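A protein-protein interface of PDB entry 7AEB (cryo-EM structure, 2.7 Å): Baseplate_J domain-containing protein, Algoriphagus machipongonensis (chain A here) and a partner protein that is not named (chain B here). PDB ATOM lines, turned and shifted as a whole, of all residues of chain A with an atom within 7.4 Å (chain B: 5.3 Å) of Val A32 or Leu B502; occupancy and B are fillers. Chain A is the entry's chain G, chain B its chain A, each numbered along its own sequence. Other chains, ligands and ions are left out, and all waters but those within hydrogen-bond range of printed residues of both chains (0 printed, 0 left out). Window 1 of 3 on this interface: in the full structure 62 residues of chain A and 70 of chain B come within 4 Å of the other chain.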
ATOM      1  N   LYS A  26     -24.291  18.324  27.457  1.00  0.00           N
ATOM      2  CA  LYS A  26     -22.942  17.813  27.307  1.00  0.00           C
ATOM      3  C   LYS A  26     -22.823  16.361  27.706  1.00  0.00           C
ATOM      4  O   LYS A  26     -21.799  15.941  28.237  1.00  0.00           O
ATOM      5  CB  LYS A  26     -21.961  18.623  28.128  1.00  0.00           C
ATOM      6  CG  LYS A  26     -21.859  20.055  27.751  1.00  0.00           C
ATOM      7  CD  LYS A  26     -20.842  20.735  28.634  1.00  0.00           C
ATOM      8  CE  LYS A  26     -20.701  22.201  28.296  1.00  0.00           C
ATOM      9  NZ  LYS A  26     -19.719  22.877  29.187  1.00  0.00           N
ATOM     10  N   ALA A  28     -24.256  13.888  25.292  1.00  0.00           N
ATOM     11  CA  ALA A  28     -24.176  13.259  23.990  1.00  0.00           C
ATOM     12  C   ALA A  28     -22.737  13.244  23.503  1.00  0.00           C
ATOM     13  O   ALA A  28     -22.092  14.297  23.506  1.00  0.00           O
ATOM     14  CB  ALA A  28     -25.037  14.008  22.990  1.00  0.00           C
ATOM     15  N   PRO A  29     -22.213  12.078  23.097  1.00  0.00           N
ATOM     16  CA  PRO A  29     -20.828  11.930  22.614  1.00  0.00           C
ATOM     17  C   PRO A  29     -20.392  12.938  21.581  1.00  0.00           C
ATOM     18  O   PRO A  29     -19.247  13.396  21.630  1.00  0.00           O
ATOM     19  CB  PRO A  29     -20.857  10.523  22.019  1.00  0.00           C
ATOM     20  CG  PRO A  29     -21.879   9.811  22.832  1.00  0.00           C
ATOM     21  CD  PRO A  29     -22.936  10.801  23.116  1.00  0.00           C
ATOM     22  N   GLU A  30     -21.311  13.386  20.735  1.00  0.00           N
ATOM     23  CA  GLU A  30     -20.946  14.306  19.670  1.00  0.00           C
ATOM     24  C   GLU A  30     -20.279  15.574  20.169  1.00  0.00           C
ATOM     25  O   GLU A  30     -19.418  16.127  19.477  1.00  0.00           O
ATOM     26  CB  GLU A  30     -22.174  14.715  18.868  1.00  0.00           C
ATOM     27  CG  GLU A  30     -21.860  15.539  17.633  1.00  0.00           C
ATOM     28  CD  GLU A  30     -23.078  15.837  16.791  1.00  0.00           C
ATOM     29  OE1 GLU A  30     -22.961  16.608  15.817  1.00  0.00           O
ATOM     30  OE2 GLU A  30     -24.184  15.400  17.177  1.00  0.00           O
ATOM     31  N   SER A  31     -20.620  16.024  21.376  1.00  0.00           N
ATOM     32  CA  SER A  31     -20.063  17.267  21.875  1.00  0.00           C
ATOM     33  C   SER A  31     -18.543  17.292  21.830  1.00  0.00           C
ATOM     34  O   SER A  31     -17.948  18.365  21.892  1.00  0.00           O
ATOM     35  CB  SER A  31     -20.535  17.494  23.301  1.00  0.00           C
ATOM     36  OG  SER A  31     -19.863  16.620  24.179  1.00  0.00           O
ATOM     37  N   VAL A  32     -17.908  16.135  21.674  1.00  0.00           N
ATOM     38  CA  VAL A  32     -16.466  16.029  21.656  1.00  0.00           C
ATOM     39  C   VAL A  32     -15.994  15.594  20.283  1.00  0.00           C
ATOM     40  O   VAL A  32     -16.319  14.495  19.824  1.00  0.00           O
ATOM     41  CB  VAL A  32     -15.983  15.042  22.712  1.00  0.00           C
ATOM     42  CG1 VAL A  32     -14.467  14.917  22.659  1.00  0.00           C
ATOM     43  CG2 VAL A  32     -16.442  15.499  24.050  1.00  0.00           C
ATOM     44  N   GLN A  33     -15.177  16.416  19.667  1.00  0.00           N
ATOM     45  CA  GLN A  33     -14.588  16.092  18.382  1.00  0.00           C
ATOM     46  C   GLN A  33     -13.109  15.893  18.624  1.00  0.00           C
ATOM     47  O   GLN A  33     -12.373  16.867  18.778  1.00  0.00           O
ATOM     48  CB  GLN A  33     -14.858  17.197  17.379  1.00  0.00           C
ATOM     49  CG  GLN A  33     -16.335  17.394  17.133  1.00  0.00           C
ATOM     50  CD  GLN A  33     -16.942  16.193  16.462  1.00  0.00           C
ATOM     51  OE1 GLN A  33     -16.387  15.698  15.491  1.00  0.00           O
ATOM     52  NE2 GLN A  33     -18.072  15.705  16.972  1.00  0.00           N
ATOM     53  N   LEU A  34     -12.688  14.630  18.669  1.00  0.00           N
ATOM     54  CA  LEU A  34     -11.311  14.307  19.019  1.00  0.00           C
ATOM     55  C   LEU A  34     -10.322  14.914  18.042  1.00  0.00           C
ATOM     56  O   LEU A  34      -9.231  15.333  18.433  1.00  0.00           O
ATOM     57  CB  LEU A  34     -11.114  12.804  19.048  1.00  0.00           C
ATOM     58  CG  LEU A  34     -11.845  12.014  20.114  1.00  0.00           C
ATOM     59  CD1 LEU A  34     -11.655  10.549  19.813  1.00  0.00           C
ATOM     60  CD2 LEU A  34     -11.318  12.357  21.480  1.00  0.00           C
ATOM     61  N   GLN A  35     -10.689  14.986  16.774  1.00  0.00           N
ATOM     62  CA  GLN A  35      -9.848  15.572  15.741  1.00  0.00           C
ATOM     63  C   GLN A  35     -10.633  16.671  15.043  1.00  0.00           C
ATOM     64  O   GLN A  35     -11.664  16.377  14.478  1.00  0.00           O
ATOM     65  CB  GLN A  35      -9.517  14.490  14.725  1.00  0.00           C
ATOM     66  CG  GLN A  35      -8.561  14.908  13.647  1.00  0.00           C
ATOM     67  CD  GLN A  35      -7.138  14.767  14.094  1.00  0.00           C
ATOM     68  OE1 GLN A  35      -6.740  13.727  14.610  1.00  0.00           O
ATOM     69  NE2 GLN A  35      -6.362  15.816  13.917  1.00  0.00           N
ATOM     70  N   ASN A 133     -13.495  10.124  14.826  1.00  0.00           N
ATOM     71  CA  ASN A 133     -14.297  10.844  15.800  1.00  0.00           C
ATOM     72  C   ASN A 133     -15.490  10.056  16.332  1.00  0.00           C
ATOM     73  O   ASN A 133     -16.228  10.591  17.157  1.00  0.00           O
ATOM     74  CB  ASN A 133     -14.764  12.162  15.201  1.00  0.00           C
ATOM     75  CG  ASN A 133     -13.675  13.206  15.205  1.00  0.00           C
ATOM     76  OD1 ASN A 133     -12.776  13.184  16.041  1.00  0.00           O
ATOM     77  ND2 ASN A 133     -13.748  14.125  14.272  1.00  0.00           N
ATOM     78  N   GLN A 134     -15.699   8.809  15.929  1.00  0.00           N
ATOM     79  CA  GLN A 134     -16.771   8.015  16.509  1.00  0.00           C
ATOM     80  C   GLN A 134     -16.312   7.221  17.715  1.00  0.00           C
ATOM     81  O   GLN A 134     -17.117   6.514  18.327  1.00  0.00           O
ATOM     82  CB  GLN A 134     -17.359   7.091  15.454  1.00  0.00           C
ATOM     83  CG  GLN A 134     -18.047   7.860  14.387  1.00  0.00           C
ATOM     84  CD  GLN A 134     -18.527   7.006  13.269  1.00  0.00           C
ATOM     85  OE1 GLN A 134     -19.383   6.138  13.439  1.00  0.00           O
ATOM     86  NE2 GLN A 134     -17.979   7.241  12.100  1.00  0.00           N
ATOM     87  N   THR A 136     -15.528   8.293  20.701  1.00  0.00           N
ATOM     88  CA  THR A 136     -16.127   8.718  21.963  1.00  0.00           C
ATOM     89  C   THR A 136     -17.444   8.021  22.225  1.00  0.00           C
ATOM     90  O   THR A 136     -17.768   7.724  23.379  1.00  0.00           O
ATOM     91  CB  THR A 136     -16.346  10.223  21.975  1.00  0.00           C
ATOM     92  OG1 THR A 136     -17.242  10.564  20.914  1.00  0.00           O
ATOM     93  CG2 THR A 136     -15.061  10.951  21.795  1.00  0.00           C
ATOM     94  N   LYS A 137     -18.200   7.740  21.170  1.00  0.00           N
ATOM     95  CA  LYS A 137     -19.461   7.048  21.354  1.00  0.00           C
ATOM     96  C   LYS A 137     -19.220   5.595  21.669  1.00  0.00           C
ATOM     97  O   LYS A 137     -19.866   5.043  22.561  1.00  0.00           O
ATOM     98  CB  LYS A 137     -20.348   7.165  20.122  1.00  0.00           C
ATOM     99  CG  LYS A 137     -21.684   6.467  20.305  1.00  0.00           C
ATOM    100  CD  LYS A 137     -22.644   6.732  19.176  1.00  0.00           C
ATOM    101  CE  LYS A 137     -23.936   5.962  19.382  1.00  0.00           C
ATOM    102  NZ  LYS A 137     -24.927   6.199  18.304  1.00  0.00           N
ATOM    103  N   LEU B 446      -6.364  10.633  27.259  1.00  0.00           N
ATOM    104  CA  LEU B 446      -7.313  11.707  27.038  1.00  0.00           C
ATOM    105  C   LEU B 446      -8.573  11.528  27.861  1.00  0.00           C
ATOM    106  O   LEU B 446      -9.120  12.503  28.376  1.00  0.00           O
ATOM    107  CB  LEU B 446      -7.659  11.775  25.558  1.00  0.00           C
ATOM    108  CG  LEU B 446      -6.536  12.259  24.626  1.00  0.00           C
ATOM    109  CD1 LEU B 446      -6.933  11.998  23.212  1.00  0.00           C
ATOM    110  CD2 LEU B 446      -6.283  13.752  24.812  1.00  0.00           C
ATOM    111  N   LEU B 447      -9.004  10.292  28.043  1.00  0.00           N
ATOM    112  CA  LEU B 447     -10.203  10.011  28.809  1.00  0.00           C
ATOM    113  C   LEU B 447      -9.946   9.444  30.212  1.00  0.00           C
ATOM    114  O   LEU B 447     -10.862   8.879  30.807  1.00  0.00           O
ATOM    115  CB  LEU B 447     -11.080   9.062  28.008  1.00  0.00           C
ATOM    116  CG  LEU B 447     -11.560   9.593  26.642  1.00  0.00           C
ATOM    117  CD1 LEU B 447     -12.307   8.510  25.940  1.00  0.00           C
ATOM    118  CD2 LEU B 447     -12.456  10.828  26.812  1.00  0.00           C
ATOM    119  N   THR B 456      -3.460  18.081  23.461  1.00  0.00           N
ATOM    120  CA  THR B 456      -4.555  17.332  22.878  1.00  0.00           C
ATOM    121  C   THR B 456      -4.203  16.832  21.483  1.00  0.00           C
ATOM    122  O   THR B 456      -4.873  15.931  20.970  1.00  0.00           O
ATOM    123  CB  THR B 456      -5.860  18.149  22.881  1.00  0.00           C
ATOM    124  OG1 THR B 456      -5.765  19.284  22.023  1.00  0.00           O
ATOM    125  CG2 THR B 456      -6.173  18.625  24.292  1.00  0.00           C
ATOM    126  N   ARG B 498      -9.877  22.849  24.733  1.00  0.00           N
ATOM    127  CA  ARG B 498     -10.099  21.444  24.462  1.00  0.00           C
ATOM    128  C   ARG B 498     -10.085  20.593  25.732  1.00  0.00           C
ATOM    129  O   ARG B 498     -10.902  19.674  25.863  1.00  0.00           O
ATOM    130  CB  ARG B 498      -9.101  20.976  23.434  1.00  0.00           C
ATOM    131  CG  ARG B 498      -9.441  21.511  22.063  1.00  0.00           C
ATOM    132  CD  ARG B 498      -8.410  21.216  21.048  1.00  0.00           C
ATOM    133  NE  ARG B 498      -8.177  19.799  20.865  1.00  0.00           N
ATOM    134  CZ  ARG B 498      -8.933  18.966  20.146  1.00  0.00           C
ATOM    135  NH1 ARG B 498     -10.029  19.389  19.543  1.00  0.00           N
ATOM    136  NH2 ARG B 498      -8.581  17.698  20.037  1.00  0.00           N
ATOM    137  N   ARG B 499      -9.194  20.895  26.673  1.00  0.00           N
ATOM    138  CA  ARG B 499      -9.156  20.140  27.909  1.00  0.00           C
ATOM    139  C   ARG B 499     -10.438  20.324  28.689  1.00  0.00           C
ATOM    140  O   ARG B 499     -10.957  19.352  29.236  1.00  0.00           O
ATOM    141  CB  ARG B 499      -7.949  20.532  28.739  1.00  0.00           C
ATOM    142  CG  ARG B 499      -6.645  20.024  28.145  1.00  0.00           C
ATOM    143  CD  ARG B 499      -5.461  20.562  28.836  1.00  0.00           C
ATOM    144  NE  ARG B 499      -5.349  20.058  30.190  1.00  0.00           N
ATOM    145  CZ  ARG B 499      -4.540  20.567  31.122  1.00  0.00           C
ATOM    146  NH1 ARG B 499      -3.762  21.597  30.849  1.00  0.00           N
ATOM    147  NH2 ARG B 499      -4.522  20.034  32.334  1.00  0.00           N
ATOM    148  N   ASN B 500     -11.002  21.532  28.697  1.00  0.00           N
ATOM    149  CA  ASN B 500     -12.259  21.702  29.401  1.00  0.00           C
ATOM    150  C   ASN B 500     -13.366  20.892  28.763  1.00  0.00           C
ATOM    151  O   ASN B 500     -14.099  20.213  29.476  1.00  0.00           O
ATOM    152  CB  ASN B 500     -12.665  23.157  29.472  1.00  0.00           C
ATOM    153  CG  ASN B 500     -11.930  23.905  30.520  1.00  0.00           C
ATOM    154  OD1 ASN B 500     -12.287  23.838  31.693  1.00  0.00           O
ATOM    155  ND2 ASN B 500     -10.914  24.615  30.137  1.00  0.00           N
ATOM    156  N   GLN B 501     -13.430  20.834  27.436  1.00  0.00           N
ATOM    157  CA  GLN B 501     -14.505  20.055  26.834  1.00  0.00           C
ATOM    158  C   GLN B 501     -14.434  18.584  27.224  1.00  0.00           C
ATOM    159  O   GLN B 501     -15.464  17.978  27.542  1.00  0.00           O
ATOM    160  CB  GLN B 501     -14.472  20.173  25.325  1.00  0.00           C
ATOM    161  CG  GLN B 501     -14.849  21.529  24.815  1.00  0.00           C
ATOM    162  CD  GLN B 501     -14.725  21.632  23.326  1.00  0.00           C
ATOM    163  OE1 GLN B 501     -14.688  20.616  22.625  1.00  0.00           O
ATOM    164  NE2 GLN B 501     -14.657  22.856  22.826  1.00  0.00           N
ATOM    165  N   LEU B 502     -13.229  18.013  27.263  1.00  0.00           N
ATOM    166  CA  LEU B 502     -13.098  16.617  27.658  1.00  0.00           C
ATOM    167  C   LEU B 502     -13.518  16.399  29.097  1.00  0.00           C
ATOM    168  O   LEU B 502     -14.227  15.435  29.405  1.00  0.00           O
ATOM    169  CB  LEU B 502     -11.656  16.140  27.506  1.00  0.00           C
ATOM    170  CG  LEU B 502     -11.088  15.955  26.093  1.00  0.00           C
ATOM    171  CD1 LEU B 502      -9.592  15.730  26.174  1.00  0.00           C
ATOM    172  CD2 LEU B 502     -11.726  14.758  25.432  1.00  0.00           C
ATOM    173  N   MET B 503     -13.107  17.299  29.986  1.00  0.00           N
ATOM    174  CA  MET B 503     -13.443  17.130  31.388  1.00  0.00           C
ATOM    175  C   MET B 503     -14.928  17.248  31.611  1.00  0.00           C
ATOM    176  O   MET B 503     -15.496  16.485  32.391  1.00  0.00           O
ATOM    177  CB  MET B 503     -12.752  18.177  32.236  1.00  0.00           C
ATOM    178  CG  MET B 503     -11.269  18.066  32.294  1.00  0.00           C
ATOM    179  SD  MET B 503     -10.696  16.505  32.829  1.00  0.00           S
ATOM    180  CE  MET B 503     -11.215  16.487  34.493  1.00  0.00           C
ATOM    181  N   ASP B 504     -15.571  18.189  30.923  1.00  0.00           N
ATOM    182  CA  ASP B 504     -16.990  18.386  31.123  1.00  0.00           C
ATOM    183  C   ASP B 504     -17.765  17.172  30.688  1.00  0.00           C
ATOM    184  O   ASP B 504     -18.718  16.780  31.363  1.00  0.00           O
ATOM    185  CB  ASP B 504     -17.480  19.616  30.382  1.00  0.00           C
ATOM    186  CG  ASP B 504     -16.999  20.917  31.018  1.00  0.00           C
ATOM    187  OD1 ASP B 504     -16.517  20.914  32.149  1.00  0.00           O
ATOM    188  OD2 ASP B 504     -17.145  21.943  30.389  1.00  0.00           O
ATOM    189  N   HIS B 505     -17.339  16.537  29.601  1.00  0.00           N
ATOM    190  CA  HIS B 505     -18.000  15.323  29.165  1.00  0.00           C
ATOM    191  C   HIS B 505     -17.900  14.237  30.224  1.00  0.00           C
ATOM    192  O   HIS B 505     -18.904  13.611  30.568  1.00  0.00           O
ATOM    193  CB  HIS B 505     -17.413  14.821  27.865  1.00  0.00           C
ATOM    194  CG  HIS B 505     -18.042  13.572  27.424  1.00  0.00           C
ATOM    195  ND1 HIS B 505     -19.303  13.523  26.891  1.00  0.00           N
ATOM    196  CD2 HIS B 505     -17.599  12.309  27.477  1.00  0.00           C
ATOM    197  CE1 HIS B 505     -19.607  12.273  26.620  1.00  0.00           C
ATOM    198  NE2 HIS B 505     -18.592  11.511  26.976  1.00  0.00           N
ATOM    199  N   LEU B 506     -16.702  14.000  30.746  1.00  0.00           N
ATOM    200  CA  LEU B 506     -16.560  12.942  31.730  1.00  0.00           C
ATOM    201  C   LEU B 506     -17.387  13.228  32.977  1.00  0.00           C
ATOM    202  O   LEU B 506     -18.009  12.324  33.528  1.00  0.00           O
ATOM    203  CB  LEU B 506     -15.098  12.775  32.124  1.00  0.00           C
ATOM    204  CG  LEU B 506     -14.118  12.251  31.060  1.00  0.00           C
ATOM    205  CD1 LEU B 506     -12.716  12.314  31.628  1.00  0.00           C
ATOM    206  CD2 LEU B 506     -14.454  10.837  30.634  1.00  0.00           C
ATOM    207  N   ILE B 507     -17.434  14.488  33.407  1.00  0.00           N
ATOM    208  CA  ILE B 507     -18.212  14.854  34.587  1.00  0.00           C
ATOM    209  C   ILE B 507     -19.693  14.624  34.342  1.00  0.00           C
ATOM    210  O   ILE B 507     -20.397  14.069  35.195  1.00  0.00           O
ATOM    211  CB  ILE B 507     -17.894  16.300  35.024  1.00  0.00           C
ATOM    212  CG1 ILE B 507     -16.451  16.338  35.576  1.00  0.00           C
ATOM    213  CG2 ILE B 507     -18.869  16.785  36.065  1.00  0.00           C
ATOM    214  CD1 ILE B 507     -15.856  17.702  35.808  1.00  0.00           C
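The side-chain amide oxygen (OD1) of Asn A133 sits at hydrogen-bond distance from the backbone NH (N) of Leu A34, 3.0 Å away. The backbone carbonyl oxygen (O) of Glu A30 is in hydrogen-bond range of the side-chain amide nitrogen (NE2) of Gln A33, 2.9 Å away. OE1 of Gln A33 sits at hydrogen-bond distance from ND2 of Asn A133 (3.3 Å). The side-chain hydroxyl (OG1) of Thr B456 lies within hydrogen-bond range of the guanidinium group (NE) of Arg B498 (2.7 Å).
Hydrophobic or aromatic side chains of chain B within 4 Å of the printed part of chain A: Leu B502 and His B505. Among the printed residues, 6 pairs touch across the chains.
O of Lys A26 touches ND1 of His B505, at 3.7 Å. Leu B502 touches Val A32. Val A32 touches His B505. O of Gln A33 touches NH1 of Arg B498, 3.5 Å away.
Of the printed residues of chain B, Val A32 touches Leu B502 (3.9 Å) and His B505 (3.99 Å). Leu B502 touches one residue of chain A. Printed residues of chain A within 4 Å of His B505: Lys A26 (3.7 Å) and Val A32 (3.99 Å). Printed residues of chain B within 4 Å of Gln A33: Arg B498. Of the printed residues of chain B, Leu A34 touches Arg B498 (2.9 Å). Of the printed residues of chain A, Arg B498 touches Gln A33 (3.5 Å) and Leu A34 (2.9 Å). Of the printed residues of chain A, Asp B504 touches Lys A26 (3.0 Å). Gln A134 touches none of the printed residues of chain B. The nearest residue of chain A that does not touch Leu B502 is Leu A34 (4.6 Å).
O of Leu A34 sits at hydrogen-bond distance from NH2 of Arg B498, at 2.9 Å. The side-chain carboxylate (OD2) of Asp B504 is in salt-bridge range of the side-chain amino group (NZ) of Lys A26, at 3.0 Å.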
